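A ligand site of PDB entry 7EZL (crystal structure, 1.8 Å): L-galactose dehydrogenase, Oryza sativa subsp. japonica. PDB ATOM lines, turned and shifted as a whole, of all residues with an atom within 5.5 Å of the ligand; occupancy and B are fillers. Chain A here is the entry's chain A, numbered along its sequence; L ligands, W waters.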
ATOM      1  N   PHE A  26     -13.993   5.047 -16.933  1.00  0.00           N
ATOM      2  CA  PHE A  26     -14.564   4.880 -18.253  1.00  0.00           C
ATOM      3  C   PHE A  26     -15.145   6.204 -18.748  1.00  0.00           C
ATOM      4  O   PHE A  26     -16.157   6.677 -18.265  1.00  0.00           O
ATOM      5  CB  PHE A  26     -15.658   3.817 -18.204  1.00  0.00           C
ATOM      6  CG  PHE A  26     -15.997   3.190 -19.542  1.00  0.00           C
ATOM      7  CD1 PHE A  26     -16.452   3.965 -20.594  1.00  0.00           C
ATOM      8  CD2 PHE A  26     -15.847   1.820 -19.746  1.00  0.00           C
ATOM      9  CE1 PHE A  26     -16.760   3.387 -21.827  1.00  0.00           C
ATOM     10  CE2 PHE A  26     -16.161   1.244 -20.963  1.00  0.00           C
ATOM     11  CZ  PHE A  26     -16.605   2.027 -22.011  1.00  0.00           C
ATOM     12  N   GLY A  27     -14.449   6.830 -19.706  1.00  0.00           N
ATOM     13  CA  GLY A  27     -15.049   7.985 -20.359  1.00  0.00           C
ATOM     14  C   GLY A  27     -15.924   7.542 -21.524  1.00  0.00           C
ATOM     15  O   GLY A  27     -15.459   6.857 -22.430  1.00  0.00           O
ATOM     16  N   ALA A  28     -17.193   7.916 -21.473  1.00  0.00           N
ATOM     17  CA  ALA A  28     -18.184   7.301 -22.349  1.00  0.00           C
ATOM     18  C   ALA A  28     -18.283   8.049 -23.680  1.00  0.00           C
ATOM     19  O   ALA A  28     -19.144   7.717 -24.505  1.00  0.00           O
ATOM     20  CB  ALA A  28     -19.492   7.224 -21.614  1.00  0.00           C
ATOM     21  N   SER A  29     -17.384   9.010 -23.909  1.00  0.00           N
ATOM     22  CA  SER A  29     -17.259   9.659 -25.210  1.00  0.00           C
ATOM     23  C   SER A  29     -15.794   9.892 -25.587  1.00  0.00           C
ATOM     24  O   SER A  29     -15.258  10.996 -25.401  1.00  0.00           O
ATOM     25  CB  SER A  29     -18.066  10.937 -25.259  1.00  0.00           C
ATOM     26  OG  SER A  29     -17.686  11.786 -24.180  1.00  0.00           O
ATOM     27  N   PRO A  30     -15.094   8.875 -26.140  1.00  0.00           N
ATOM     28  CA  PRO A  30     -13.753   9.064 -26.718  1.00  0.00           C
ATOM     29  C   PRO A  30     -13.666   9.905 -27.996  1.00  0.00           C
ATOM     30  O   PRO A  30     -14.349   9.621 -28.988  1.00  0.00           O
ATOM     31  CB  PRO A  30     -13.315   7.612 -27.024  1.00  0.00           C
ATOM     32  CG  PRO A  30     -14.609   6.865 -27.228  1.00  0.00           C
ATOM     33  CD  PRO A  30     -15.545   7.468 -26.203  1.00  0.00           C
ATOM     34  N   LEU A  31     -12.808  10.943 -27.976  1.00  0.00           N
ATOM     35  CA  LEU A  31     -12.543  11.864 -29.084  1.00  0.00           C
ATOM     36  C   LEU A  31     -13.822  12.610 -29.510  1.00  0.00           C
ATOM     37  O   LEU A  31     -14.033  12.834 -30.697  1.00  0.00           O
ATOM     38  CB  LEU A  31     -11.950  11.115 -30.289  1.00  0.00           C
ATOM     39  CG  LEU A  31     -10.554  10.488 -30.121  1.00  0.00           C
ATOM     40  CD1 LEU A  31     -10.006  10.048 -31.477  1.00  0.00           C
ATOM     41  CD2 LEU A  31      -9.586  11.444 -29.428  1.00  0.00           C
ATOM     42  N   GLY A  32     -14.665  12.992 -28.529  1.00  0.00           N
ATOM     43  CA  GLY A  32     -15.871  13.752 -28.813  1.00  0.00           C
ATOM     44  C   GLY A  32     -16.883  13.001 -29.678  1.00  0.00           C
ATOM     45  O   GLY A  32     -17.527  13.602 -30.548  1.00  0.00           O
ATOM     46  N   ASP A  59     -18.086   8.256 -16.601  1.00  0.00           N
ATOM     47  CA  ASP A  59     -18.257   9.670 -16.879  1.00  0.00           C
ATOM     48  C   ASP A  59     -18.940   9.865 -18.225  1.00  0.00           C
ATOM     49  O   ASP A  59     -18.547   9.257 -19.227  1.00  0.00           O
ATOM     50  CB  ASP A  59     -16.903  10.395 -16.824  1.00  0.00           C
ATOM     51  CG  ASP A  59     -17.044  11.886 -17.000  1.00  0.00           C
ATOM     52  OD1 ASP A  59     -17.473  12.545 -16.028  1.00  0.00           O
ATOM     53  OD2 ASP A  59     -16.727  12.380 -18.116  1.00  0.00           O
ATOM     54  N   THR A  60     -19.930  10.765 -18.250  1.00  0.00           N
ATOM     55  CA  THR A  60     -20.634  11.123 -19.472  1.00  0.00           C
ATOM     56  C   THR A  60     -21.030  12.595 -19.381  1.00  0.00           C
ATOM     57  O   THR A  60     -20.572  13.313 -18.483  1.00  0.00           O
ATOM     58  CB  THR A  60     -21.875  10.249 -19.693  1.00  0.00           C
ATOM     59  OG1 THR A  60     -22.392  10.579 -20.991  1.00  0.00           O
ATOM     60  CG2 THR A  60     -22.910  10.419 -18.608  1.00  0.00           C
ATOM     61  N   TYR A  64     -21.652  15.397 -25.811  1.00  0.00           N
ATOM     62  CA  TYR A  64     -21.086  14.683 -26.955  1.00  0.00           C
ATOM     63  C   TYR A  64     -22.129  13.729 -27.522  1.00  0.00           C
ATOM     64  O   TYR A  64     -22.669  12.903 -26.777  1.00  0.00           O
ATOM     65  CB  TYR A  64     -19.779  13.973 -26.589  1.00  0.00           C
ATOM     66  CG  TYR A  64     -18.689  14.962 -26.293  1.00  0.00           C
ATOM     67  CD1 TYR A  64     -18.197  15.761 -27.318  1.00  0.00           C
ATOM     68  CD2 TYR A  64     -18.176  15.142 -25.020  1.00  0.00           C
ATOM     69  CE1 TYR A  64     -17.214  16.701 -27.087  1.00  0.00           C
ATOM     70  CE2 TYR A  64     -17.199  16.098 -24.775  1.00  0.00           C
ATOM     71  CZ  TYR A  64     -16.718  16.880 -25.815  1.00  0.00           C
ATOM     72  OH  TYR A  64     -15.752  17.822 -25.621  1.00  0.00           O
ATOM     73  N   LYS A  92     -22.728  15.953 -16.417  1.00  0.00           N
ATOM     74  CA  LYS A  92     -22.387  17.361 -16.412  1.00  0.00           C
ATOM     75  C   LYS A  92     -23.600  18.167 -16.845  1.00  0.00           C
ATOM     76  O   LYS A  92     -24.560  17.601 -17.368  1.00  0.00           O
ATOM     77  CB  LYS A  92     -21.176  17.547 -17.329  1.00  0.00           C
ATOM     78  CG  LYS A  92     -20.086  16.487 -17.128  1.00  0.00           C
ATOM     79  CD  LYS A  92     -18.782  16.858 -17.843  1.00  0.00           C
ATOM     80  CE  LYS A  92     -17.708  15.800 -17.803  1.00  0.00           C
ATOM     81  NZ  LYS A  92     -18.050  14.607 -18.601  1.00  0.00           N
ATOM     82  N   HIS A 129     -19.787  22.030 -16.785  1.00  0.00           N
ATOM     83  CA  HIS A 129     -19.016  21.493 -17.901  1.00  0.00           C
ATOM     84  C   HIS A 129     -18.256  22.626 -18.624  1.00  0.00           C
ATOM     85  O   HIS A 129     -18.889  23.513 -19.177  1.00  0.00           O
ATOM     86  CB  HIS A 129     -19.974  20.836 -18.904  1.00  0.00           C
ATOM     87  CG  HIS A 129     -19.350  19.891 -19.856  1.00  0.00           C
ATOM     88  ND1 HIS A 129     -20.101  18.992 -20.573  1.00  0.00           N
ATOM     89  CD2 HIS A 129     -18.054  19.687 -20.173  1.00  0.00           C
ATOM     90  CE1 HIS A 129     -19.288  18.272 -21.323  1.00  0.00           C
ATOM     91  NE2 HIS A 129     -18.010  18.660 -21.067  1.00  0.00           N
ATOM     92  N   ASP A 130     -16.914  22.514 -18.717  1.00  0.00           N
ATOM     93  CA  ASP A 130     -16.118  23.434 -19.517  1.00  0.00           C
ATOM     94  C   ASP A 130     -16.486  24.869 -19.135  1.00  0.00           C
ATOM     95  O   ASP A 130     -16.932  25.641 -19.972  1.00  0.00           O
ATOM     96  CB  ASP A 130     -16.340  23.144 -21.012  1.00  0.00           C
ATOM     97  CG  ASP A 130     -15.735  21.814 -21.452  1.00  0.00           C
ATOM     98  OD1 ASP A 130     -14.825  21.356 -20.763  1.00  0.00           O
ATOM     99  OD2 ASP A 130     -16.154  21.252 -22.499  1.00  0.00           O
ATOM    100  N   THR A 162     -15.390  21.412 -14.285  1.00  0.00           N
ATOM    101  CA  THR A 162     -14.502  20.830 -15.292  1.00  0.00           C
ATOM    102  C   THR A 162     -14.168  21.882 -16.344  1.00  0.00           C
ATOM    103  O   THR A 162     -14.847  22.910 -16.457  1.00  0.00           O
ATOM    104  CB  THR A 162     -15.122  19.648 -16.057  1.00  0.00           C
ATOM    105  OG1 THR A 162     -15.656  19.986 -17.344  1.00  0.00           O
ATOM    106  CG2 THR A 162     -16.131  18.845 -15.272  1.00  0.00           C
ATOM    107  N   GLY A 163     -13.169  21.577 -17.163  1.00  0.00           N
ATOM    108  CA  GLY A 163     -12.628  22.520 -18.134  1.00  0.00           C
ATOM    109  C   GLY A 163     -11.155  22.253 -18.404  1.00  0.00           C
ATOM    110  O   GLY A 163     -10.575  21.379 -17.767  1.00  0.00           O
ATOM    111  N   LEU A 164     -10.551  22.988 -19.351  1.00  0.00           N
ATOM    112  CA  LEU A 164      -9.174  22.689 -19.734  1.00  0.00           C
ATOM    113  C   LEU A 164      -8.136  23.521 -18.972  1.00  0.00           C
ATOM    114  O   LEU A 164      -7.179  22.949 -18.434  1.00  0.00           O
ATOM    115  CB  LEU A 164      -9.009  22.852 -21.246  1.00  0.00           C
ATOM    116  CG  LEU A 164      -7.574  22.568 -21.708  1.00  0.00           C
ATOM    117  CD1 LEU A 164      -7.276  21.069 -21.616  1.00  0.00           C
ATOM    118  CD2 LEU A 164      -7.316  23.131 -23.125  1.00  0.00           C
ATOM    119  N   LEU A 185     -12.804  17.856 -12.416  1.00  0.00           N
ATOM    120  CA  LEU A 185     -12.364  17.012 -13.514  1.00  0.00           C
ATOM    121  C   LEU A 185     -11.467  17.885 -14.390  1.00  0.00           C
ATOM    122  O   LEU A 185     -11.902  18.951 -14.838  1.00  0.00           O
ATOM    123  CB  LEU A 185     -13.602  16.490 -14.268  1.00  0.00           C
ATOM    124  CG  LEU A 185     -13.341  15.281 -15.175  1.00  0.00           C
ATOM    125  CD1 LEU A 185     -14.650  14.761 -15.758  1.00  0.00           C
ATOM    126  CD2 LEU A 185     -12.404  15.658 -16.298  1.00  0.00           C
ATOM    127  N   TYR A 187      -8.556  17.649 -17.722  1.00  0.00           N
ATOM    128  CA  TYR A 187      -8.123  16.712 -18.752  1.00  0.00           C
ATOM    129  C   TYR A 187      -6.921  17.257 -19.522  1.00  0.00           C
ATOM    130  O   TYR A 187      -6.672  18.441 -19.505  1.00  0.00           O
ATOM    131  CB  TYR A 187      -9.262  16.405 -19.731  1.00  0.00           C
ATOM    132  CG  TYR A 187      -9.685  17.534 -20.638  1.00  0.00           C
ATOM    133  CD1 TYR A 187     -10.473  18.586 -20.176  1.00  0.00           C
ATOM    134  CD2 TYR A 187      -9.339  17.513 -21.979  1.00  0.00           C
ATOM    135  CE1 TYR A 187     -10.868  19.607 -21.037  1.00  0.00           C
ATOM    136  CE2 TYR A 187      -9.727  18.524 -22.867  1.00  0.00           C
ATOM    137  CZ  TYR A 187     -10.486  19.574 -22.376  1.00  0.00           C
ATOM    138  OH  TYR A 187     -10.866  20.527 -23.275  1.00  0.00           O
ATOM    139  N   ALA A 214      -8.310  13.226 -16.871  1.00  0.00           N
ATOM    140  CA  ALA A 214      -8.880  12.577 -18.046  1.00  0.00           C
ATOM    141  C   ALA A 214      -7.940  12.784 -19.219  1.00  0.00           C
ATOM    142  O   ALA A 214      -7.081  13.689 -19.179  1.00  0.00           O
ATOM    143  CB  ALA A 214     -10.257  13.170 -18.345  1.00  0.00           C
ATOM    144  N   SER A 215      -8.193  12.034 -20.304  1.00  0.00           N
ATOM    145  CA  SER A 215      -7.427  12.161 -21.541  1.00  0.00           C
ATOM    146  C   SER A 215      -5.941  11.890 -21.281  1.00  0.00           C
ATOM    147  O   SER A 215      -5.098  12.721 -21.635  1.00  0.00           O
ATOM    148  CB  SER A 215      -7.564  13.507 -22.165  1.00  0.00           C
ATOM    149  OG  SER A 215      -8.921  13.843 -22.414  1.00  0.00           O
ATOM    150  N   PRO A 216      -5.582  10.728 -20.704  1.00  0.00           N
ATOM    151  CA  PRO A 216      -4.195  10.374 -20.448  1.00  0.00           C
ATOM    152  C   PRO A 216      -3.385  10.217 -21.747  1.00  0.00           C
ATOM    153  O   PRO A 216      -2.143  10.328 -21.718  1.00  0.00           O
ATOM    154  CB  PRO A 216      -4.283   8.995 -19.750  1.00  0.00           C
ATOM    155  CG  PRO A 216      -5.607   8.404 -20.202  1.00  0.00           C
ATOM    156  CD  PRO A 216      -6.508   9.610 -20.396  1.00  0.00           C
ATOM    157  N   LEU A 217      -4.075   9.974 -22.875  1.00  0.00           N
ATOM    158  CA  LEU A 217      -3.396   9.883 -24.166  1.00  0.00           C
ATOM    159  C   LEU A 217      -3.422  11.225 -24.878  1.00  0.00           C
ATOM    160  O   LEU A 217      -3.129  11.331 -26.078  1.00  0.00           O
ATOM    161  CB  LEU A 217      -4.073   8.816 -25.020  1.00  0.00           C
ATOM    162  CG  LEU A 217      -4.267   7.466 -24.339  1.00  0.00           C
ATOM    163  CD1 LEU A 217      -4.918   6.473 -25.307  1.00  0.00           C
ATOM    164  CD2 LEU A 217      -2.936   6.943 -23.785  1.00  0.00           C
ATOM    165  N   ALA A 218      -3.887  12.265 -24.173  1.00  0.00           N
ATOM    166  CA  ALA A 218      -3.983  13.607 -24.738  1.00  0.00           C
ATOM    167  C   ALA A 218      -4.843  13.644 -26.011  1.00  0.00           C
ATOM    168  O   ALA A 218      -4.514  14.340 -26.994  1.00  0.00           O
ATOM    169  CB  ALA A 218      -2.598  14.226 -24.946  1.00  0.00           C
ATOM    170  N   MET A 219      -5.960  12.913 -25.971  1.00  0.00           N
ATOM    171  CA  MET A 219      -6.940  12.896 -27.043  1.00  0.00           C
ATOM    172  C   MET A 219      -6.334  12.318 -28.321  1.00  0.00           C
ATOM    173  O   MET A 219      -6.626  12.760 -29.435  1.00  0.00           O
ATOM    174  CB  MET A 219      -7.573  14.274 -27.290  1.00  0.00           C
ATOM    175  CG  MET A 219      -8.074  14.929 -26.011  1.00  0.00           C
ATOM    176  SD  MET A 219      -9.099  16.421 -26.273  1.00  0.00           S
ATOM    177  CE  MET A 219      -7.918  17.571 -26.971  1.00  0.00           C
ATOM    178  N   GLY A 220      -5.483  11.300 -28.144  1.00  0.00           N
ATOM    179  CA  GLY A 220      -4.927  10.572 -29.278  1.00  0.00           C
ATOM    180  C   GLY A 220      -3.494  10.971 -29.683  1.00  0.00           C
ATOM    181  O   GLY A 220      -2.941  10.362 -30.588  1.00  0.00           O
ATOM    182  N   THR A 223      -0.741   7.831 -29.231  1.00  0.00           N
ATOM    183  CA  THR A 223      -1.243   6.592 -29.799  1.00  0.00           C
ATOM    184  C   THR A 223      -0.458   6.366 -31.082  1.00  0.00           C
ATOM    185  O   THR A 223       0.079   7.325 -31.661  1.00  0.00           O
ATOM    186  CB  THR A 223      -2.732   6.698 -30.193  1.00  0.00           C
ATOM    187  OG1 THR A 223      -2.869   7.783 -31.107  1.00  0.00           O
ATOM    188  CG2 THR A 223      -3.666   6.923 -29.040  1.00  0.00           C
ATOM    189  N   ASN A 254       4.579  -0.217 -27.011  1.00  0.00           N
ATOM    190  CA  ASN A 254       3.330   0.479 -27.268  1.00  0.00           C
ATOM    191  C   ASN A 254       3.216   1.746 -26.423  1.00  0.00           C
ATOM    192  O   ASN A 254       3.134   1.697 -25.194  1.00  0.00           O
ATOM    193  CB  ASN A 254       2.093  -0.414 -27.096  1.00  0.00           C
ATOM    194  CG  ASN A 254       0.804   0.362 -27.263  1.00  0.00           C
ATOM    195  OD1 ASN A 254       0.647   1.159 -28.195  1.00  0.00           O
ATOM    196  ND2 ASN A 254      -0.117   0.162 -26.349  1.00  0.00           N
ATOM    197  N   THR A 256       0.710   3.719 -26.159  1.00  0.00           N
ATOM    198  CA  THR A 256      -0.574   3.857 -25.485  1.00  0.00           C
ATOM    199  C   THR A 256      -0.472   3.266 -24.093  1.00  0.00           C
ATOM    200  O   THR A 256      -0.927   3.860 -23.119  1.00  0.00           O
ATOM    201  CB  THR A 256      -1.746   3.265 -26.264  1.00  0.00           C
ATOM    202  OG1 THR A 256      -1.878   4.073 -27.422  1.00  0.00           O
ATOM    203  CG2 THR A 256      -3.039   3.345 -25.476  1.00  0.00           C
ATOM    204  N   LEU A 273      -9.843   9.019 -16.314  1.00  0.00           N
ATOM    205  CA  LEU A 273     -10.823   8.676 -17.311  1.00  0.00           C
ATOM    206  C   LEU A 273     -10.151   8.498 -18.671  1.00  0.00           C
ATOM    207  O   LEU A 273      -9.485   9.423 -19.174  1.00  0.00           O
ATOM    208  CB  LEU A 273     -11.915   9.744 -17.378  1.00  0.00           C
ATOM    209  CG  LEU A 273     -12.779   9.843 -16.118  1.00  0.00           C
ATOM    210  CD1 LEU A 273     -13.538  11.174 -16.099  1.00  0.00           C
ATOM    211  CD2 LEU A 273     -13.764   8.676 -16.093  1.00  0.00           C
ATOM    212  N   VAL A 274     -10.385   7.329 -19.252  1.00  0.00           N
ATOM    213  CA  VAL A 274      -9.900   6.989 -20.579  1.00  0.00           C
ATOM    214  C   VAL A 274     -11.119   6.755 -21.440  1.00  0.00           C
ATOM    215  O   VAL A 274     -12.018   5.990 -21.057  1.00  0.00           O
ATOM    216  CB  VAL A 274      -9.079   5.688 -20.671  1.00  0.00           C
ATOM    217  CG1 VAL A 274      -8.035   5.776 -21.752  1.00  0.00           C
ATOM    218  CG2 VAL A 274      -8.552   5.167 -19.364  1.00  0.00           C
ATOM    219  N   GLY A 275     -11.115   7.392 -22.606  1.00  0.00           N
ATOM    220  CA  GLY A 275     -12.146   7.125 -23.592  1.00  0.00           C
ATOM    221  C   GLY A 275     -11.924   5.737 -24.175  1.00  0.00           C
ATOM    222  O   GLY A 275     -10.793   5.398 -24.540  1.00  0.00           O
ATOM    223  N   MET A 276     -12.986   4.939 -24.188  1.00  0.00           N
ATOM    224  CA  MET A 276     -12.908   3.542 -24.596  1.00  0.00           C
ATOM    225  C   MET A 276     -14.186   3.203 -25.363  1.00  0.00           C
ATOM    226  O   MET A 276     -15.261   3.696 -25.047  1.00  0.00           O
ATOM    227  CB  MET A 276     -12.746   2.613 -23.390  1.00  0.00           C
ATOM    228  CG  MET A 276     -11.332   2.579 -22.833  1.00  0.00           C
ATOM    229  SD  MET A 276     -11.165   1.716 -21.237  1.00  0.00           S
ATOM    230  CE  MET A 276     -12.290   2.613 -20.175  1.00  0.00           C
ATOM    231  N   ASN A 277     -14.029   2.365 -26.400  1.00  0.00           N
ATOM    232  CA  ASN A 277     -15.098   2.156 -27.368  1.00  0.00           C
ATOM    233  C   ASN A 277     -15.406   0.673 -27.483  1.00  0.00           C
ATOM    234  O   ASN A 277     -16.428   0.303 -28.067  1.00  0.00           O
ATOM    235  CB  ASN A 277     -14.794   2.815 -28.721  1.00  0.00           C
ATOM    236  CG  ASN A 277     -13.455   2.410 -29.319  1.00  0.00           C
ATOM    237  OD1 ASN A 277     -12.794   3.218 -29.973  1.00  0.00           O
ATOM    238  ND2 ASN A 277     -13.055   1.169 -29.139  1.00  0.00           N
ATOM    239  N   GLN A 281     -10.378  -2.473 -25.689  1.00  0.00           N
ATOM    240  CA  GLN A 281      -9.680  -1.325 -25.133  1.00  0.00           C
ATOM    241  C   GLN A 281      -9.758  -1.362 -23.613  1.00  0.00           C
ATOM    242  O   GLN A 281      -8.777  -1.092 -22.949  1.00  0.00           O
ATOM    243  CB  GLN A 281     -10.185  -0.007 -25.717  1.00  0.00           C
ATOM    244  CG  GLN A 281      -9.792   0.189 -27.172  1.00  0.00           C
ATOM    245  CD  GLN A 281     -10.060   1.607 -27.616  1.00  0.00           C
ATOM    246  OE1 GLN A 281     -10.882   2.302 -27.016  1.00  0.00           O
ATOM    247  NE2 GLN A 281      -9.330   2.040 -28.642  1.00  0.00           N
ATOM    248  N   GLU A 284      -7.153  -3.875 -22.479  1.00  0.00           N
ATOM    249  CA  GLU A 284      -5.785  -3.382 -22.533  1.00  0.00           C
ATOM    250  C   GLU A 284      -5.499  -2.403 -21.395  1.00  0.00           C
ATOM    251  O   GLU A 284      -4.421  -2.413 -20.854  1.00  0.00           O
ATOM    252  CB  GLU A 284      -5.459  -2.803 -23.913  1.00  0.00           C
ATOM    253  CG  GLU A 284      -5.302  -3.879 -24.977  1.00  0.00           C
ATOM    254  CD  GLU A 284      -5.388  -3.356 -26.406  1.00  0.00           C
ATOM    255  OE1 GLU A 284      -5.429  -2.124 -26.587  1.00  0.00           O
ATOM    256  OE2 GLU A 284      -5.412  -4.190 -27.330  1.00  0.00           O
ATOM    257  N   ASN A 285      -6.462  -1.514 -21.094  1.00  0.00           N
ATOM    258  CA  ASN A 285      -6.235  -0.469 -20.097  1.00  0.00           C
ATOM    259  C   ASN A 285      -6.290  -1.051 -18.683  1.00  0.00           C
ATOM    260  O   ASN A 285      -5.506  -0.690 -17.822  1.00  0.00           O
ATOM    261  CB  ASN A 285      -7.221   0.697 -20.300  1.00  0.00           C
ATOM    262  CG  ASN A 285      -7.019   1.433 -21.618  1.00  0.00           C
ATOM    263  OD1 ASN A 285      -7.918   2.098 -22.125  1.00  0.00           O
ATOM    264  ND2 ASN A 285      -5.861   1.267 -22.225  1.00  0.00           N
HETATM  265  P1  LIG L   1      -7.914  10.060 -24.358  1.00  0.00           P
HETATM  266  O1  LIG L   1      -6.627  10.748 -24.287  1.00  0.00           O
HETATM  267  O2  LIG L   1      -8.598   9.287 -23.264  1.00  0.00           O
HETATM  268  O3  LIG L   1      -7.857   9.169 -25.686  1.00  0.00           O
HETATM  269  C1  LIG L   1      -8.987   8.419 -26.125  1.00  0.00           C
HETATM  270  C2  LIG L   1      -8.633   7.814 -27.457  1.00  0.00           C
HETATM  271  O4  LIG L   1      -7.631   6.769 -27.271  1.00  0.00           O
HETATM  272  C3  LIG L   1      -9.802   7.169 -28.204  1.00  0.00           C
HETATM  273  O5  LIG L   1      -9.670   7.495 -29.584  1.00  0.00           O
HETATM  274  C4  LIG L   1      -9.628   5.691 -27.808  1.00  0.00           C
HETATM  275  O6  LIG L   1     -10.324   4.745 -28.593  1.00  0.00           O
HETATM  276  C5  LIG L   1      -8.112   5.552 -27.784  1.00  0.00           C
HETATM  277  N1  LIG L   1      -7.639   4.471 -26.919  1.00  0.00           N
HETATM  278  C6  LIG L   1      -7.984   4.268 -25.607  1.00  0.00           C
HETATM  279  N2  LIG L   1      -7.423   3.210 -25.088  1.00  0.00           N
HETATM  280  C7  LIG L   1      -6.664   2.668 -26.122  1.00  0.00           C
HETATM  281  C8  LIG L   1      -5.840   1.533 -26.204  1.00  0.00           C
HETATM  282  N3  LIG L   1      -5.630   0.699 -25.181  1.00  0.00           N
HETATM  283  N4  LIG L   1      -5.239   1.272 -27.390  1.00  0.00           N
HETATM  284  C9  LIG L   1      -5.450   2.106 -28.413  1.00  0.00           C
HETATM  285  N5  LIG L   1      -6.208   3.210 -28.446  1.00  0.00           N
HETATM  286  C10 LIG L   1      -6.801   3.436 -27.259  1.00  0.00           C
HETATM  287  O7  LIG L   1      -9.030  11.205 -24.676  1.00  0.00           O
HETATM  288  P2  LIG L   1     -10.594  11.425 -24.409  1.00  0.00           P
HETATM  289  O8  LIG L   1     -11.316  10.149 -24.697  1.00  0.00           O
HETATM  290  O9  LIG L   1     -10.935  12.633 -25.213  1.00  0.00           O
HETATM  291  O10 LIG L   1     -10.721  11.755 -22.838  1.00  0.00           O
HETATM  292  C11 LIG L   1     -11.203  10.685 -21.938  1.00  0.00           C
HETATM  293  C12 LIG L   1     -12.522  11.048 -21.273  1.00  0.00           C
HETATM  294  O11 LIG L   1     -12.282  12.179 -20.409  1.00  0.00           O
HETATM  295  C13 LIG L   1     -13.741  11.470 -22.135  1.00  0.00           C
HETATM  296  O12 LIG L   1     -14.532  10.447 -22.744  1.00  0.00           O
HETATM  297  C14 LIG L   1     -14.547  12.241 -21.079  1.00  0.00           C
HETATM  298  O13 LIG L   1     -15.338  11.444 -20.202  1.00  0.00           O
HETATM  299  C15 LIG L   1     -13.469  12.954 -20.254  1.00  0.00           C
HETATM  300  N6  LIG L   1     -13.182  14.368 -20.678  1.00  0.00           N
HETATM  301  C16 LIG L   1     -13.729  15.413 -19.953  1.00  0.00           C
HETATM  302  C17 LIG L   1     -13.668  16.728 -20.439  1.00  0.00           C
HETATM  303  C18 LIG L   1     -14.309  17.787 -19.553  1.00  0.00           C
HETATM  304  O14 LIG L   1     -14.997  17.439 -18.607  1.00  0.00           O
HETATM  305  N7  LIG L   1     -14.104  19.072 -19.816  1.00  0.00           N
HETATM  306  C19 LIG L   1     -13.063  16.936 -21.700  1.00  0.00           C
HETATM  307  C20 LIG L   1     -12.288  15.927 -22.281  1.00  0.00           C
HETATM  308  C21 LIG L   1     -12.374  14.648 -21.771  1.00  0.00           C
HETATM  309  O   HOH W   1     -15.365  18.395 -22.603  1.00  0.00           O
HETATM  310  O   HOH W   2      -6.142   4.612 -30.922  1.00  0.00           O
HETATM  311  O   HOH W   3      -3.384  -0.514 -27.709  1.00  0.00           O
HETATM  312  O   HOH W   4      -2.455  -0.556 -24.889  1.00  0.00           O
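OD1 of Asp 130 is in hydrogen-bond range of N7 of the ligand (2.6 Å).
The side-chain carboxylate (OD2) of Asp 59 sits at hydrogen-bond distance from an oxygen (O13) of the ligand, 2.7 Å away.
The side-chain hydroxyl (OG) of Ser 215 lies within hydrogen-bond range of an oxygen (O10) of the ligand (2.8 Å).
The backbone NH (N) of Ser 29 sits close to an oxygen (O12) of the ligand (3.4 Å).
The backbone carbonyl oxygen (O) of Ser 29 is in hydrogen-bond range of an oxygen (O12) of the ligand (2.8 Å).
N of Met 219 sits at hydrogen-bond distance from O1 of the ligand (2.8 Å).
The side-chain amide nitrogen of Gln 281 lies within hydrogen-bond range of an oxygen (O6) of the ligand (2.9 Å).
The side-chain hydroxyl (OG1) of Thr 162 is in hydrogen-bond range of an oxygen (O14) of the ligand (2.9 Å).
The backbone NH (N) of Leu 217 sits at hydrogen-bond distance from an oxygen (O1) of the ligand, at 3.0 Å.
N3 of the ligand lies close to ND2 of Asn 285, at 3.0 Å.
The backbone NH of Ala 218 lies within hydrogen-bond range of an oxygen (O1) of the ligand, at 3.1 Å.
The side-chain carboxylate of Glu 284 is in hydrogen-bond range of a nitrogen (N3) of the ligand, 3.2 Å away.
N of Gly 275 sits at hydrogen-bond distance from O2 of the ligand (3.2 Å).
The side-chain amide oxygen (OD1) of Asn 277 lies within hydrogen-bond range of an oxygen (O6) of the ligand.
The side-chain carboxylate of Asp 130 sits close to a ring nitrogen (NE2) of His 129 (3.5 Å).
The side-chain carboxylate (OD2) of Asp 59 is in salt-bridge range of the side-chain amino group (NZ) of Lys 92.
O of Asp 59 sits at hydrogen-bond distance from N of Ala 28.
The backbone NH of Asp 59 lies within hydrogen-bond range of the backbone carbonyl oxygen of Phe 26, 3.0 Å away.
The backbone carbonyl oxygen of Leu 273 lies within hydrogen-bond range of the backbone NH of Ser 215, at 3.1 Å.
The side-chain amide oxygen of Gln 281 is in hydrogen-bond range of the backbone NH of Asn 277.
The backbone carbonyl oxygen (O) of Thr 60 sits at hydrogen-bond distance from the side-chain amino group (NZ) of Lys 92 (2.8 Å).
The backbone NH (N) of Thr 256 lies close to the side-chain amide oxygen (OD1) of Asn 254, 3.3 Å away.
Gly 27 touches the ligand.
Ala 28 touches the ligand.
Pro 30 touches the ligand.
Leu 31 touches the ligand.
Lys 92 touches the ligand.
Gly 163 touches the ligand.
CD2 of Leu 185 touches C16 of the ligand, 3.9 Å away.
Tyr 187 touches the ligand.
CB of Ala 214 touches O11 of the ligand, 3.1 Å away.
CD of Pro 216 touches O2 of the ligand (3.6 Å).
CG2 of Thr 256 touches C8 of the ligand, at 3.4 Å.
O of Leu 273 touches C11 of the ligand (3.5 Å).
Val 274 touches the ligand (CA to O2, 3.8 Å).
Hydrophobic or aromatic side chains within 4 Å of the ligand: Pro 30, Leu 31, Leu 185, Tyr 187, Ala 214, Pro 216, Leu 217, Met 219, Leu 273 and Val 274.
Of the 36 residues printed, 26 come within 4 Å of the ligand.
The nearest printed residue that does not touch the ligand is His 129 (4.01 Å).
Water W3 bridges a nitrogen (N4) of the ligand and the side-chain carboxylate of Glu 284.
Water W1 lies within hydrogen-bond range of OD2 of Asp 130 (3.0 Å), NE2 of His 129 (3.1 Å), OH of Tyr 64 (3.1 Å) and N7 of the ligand (3.1 Å).
Water W4 lies within hydrogen-bond range of the side-chain amide nitrogen (ND2) of Asn 254 (2.8 Å) and a nitrogen (N3) of the ligand (3.4 Å).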
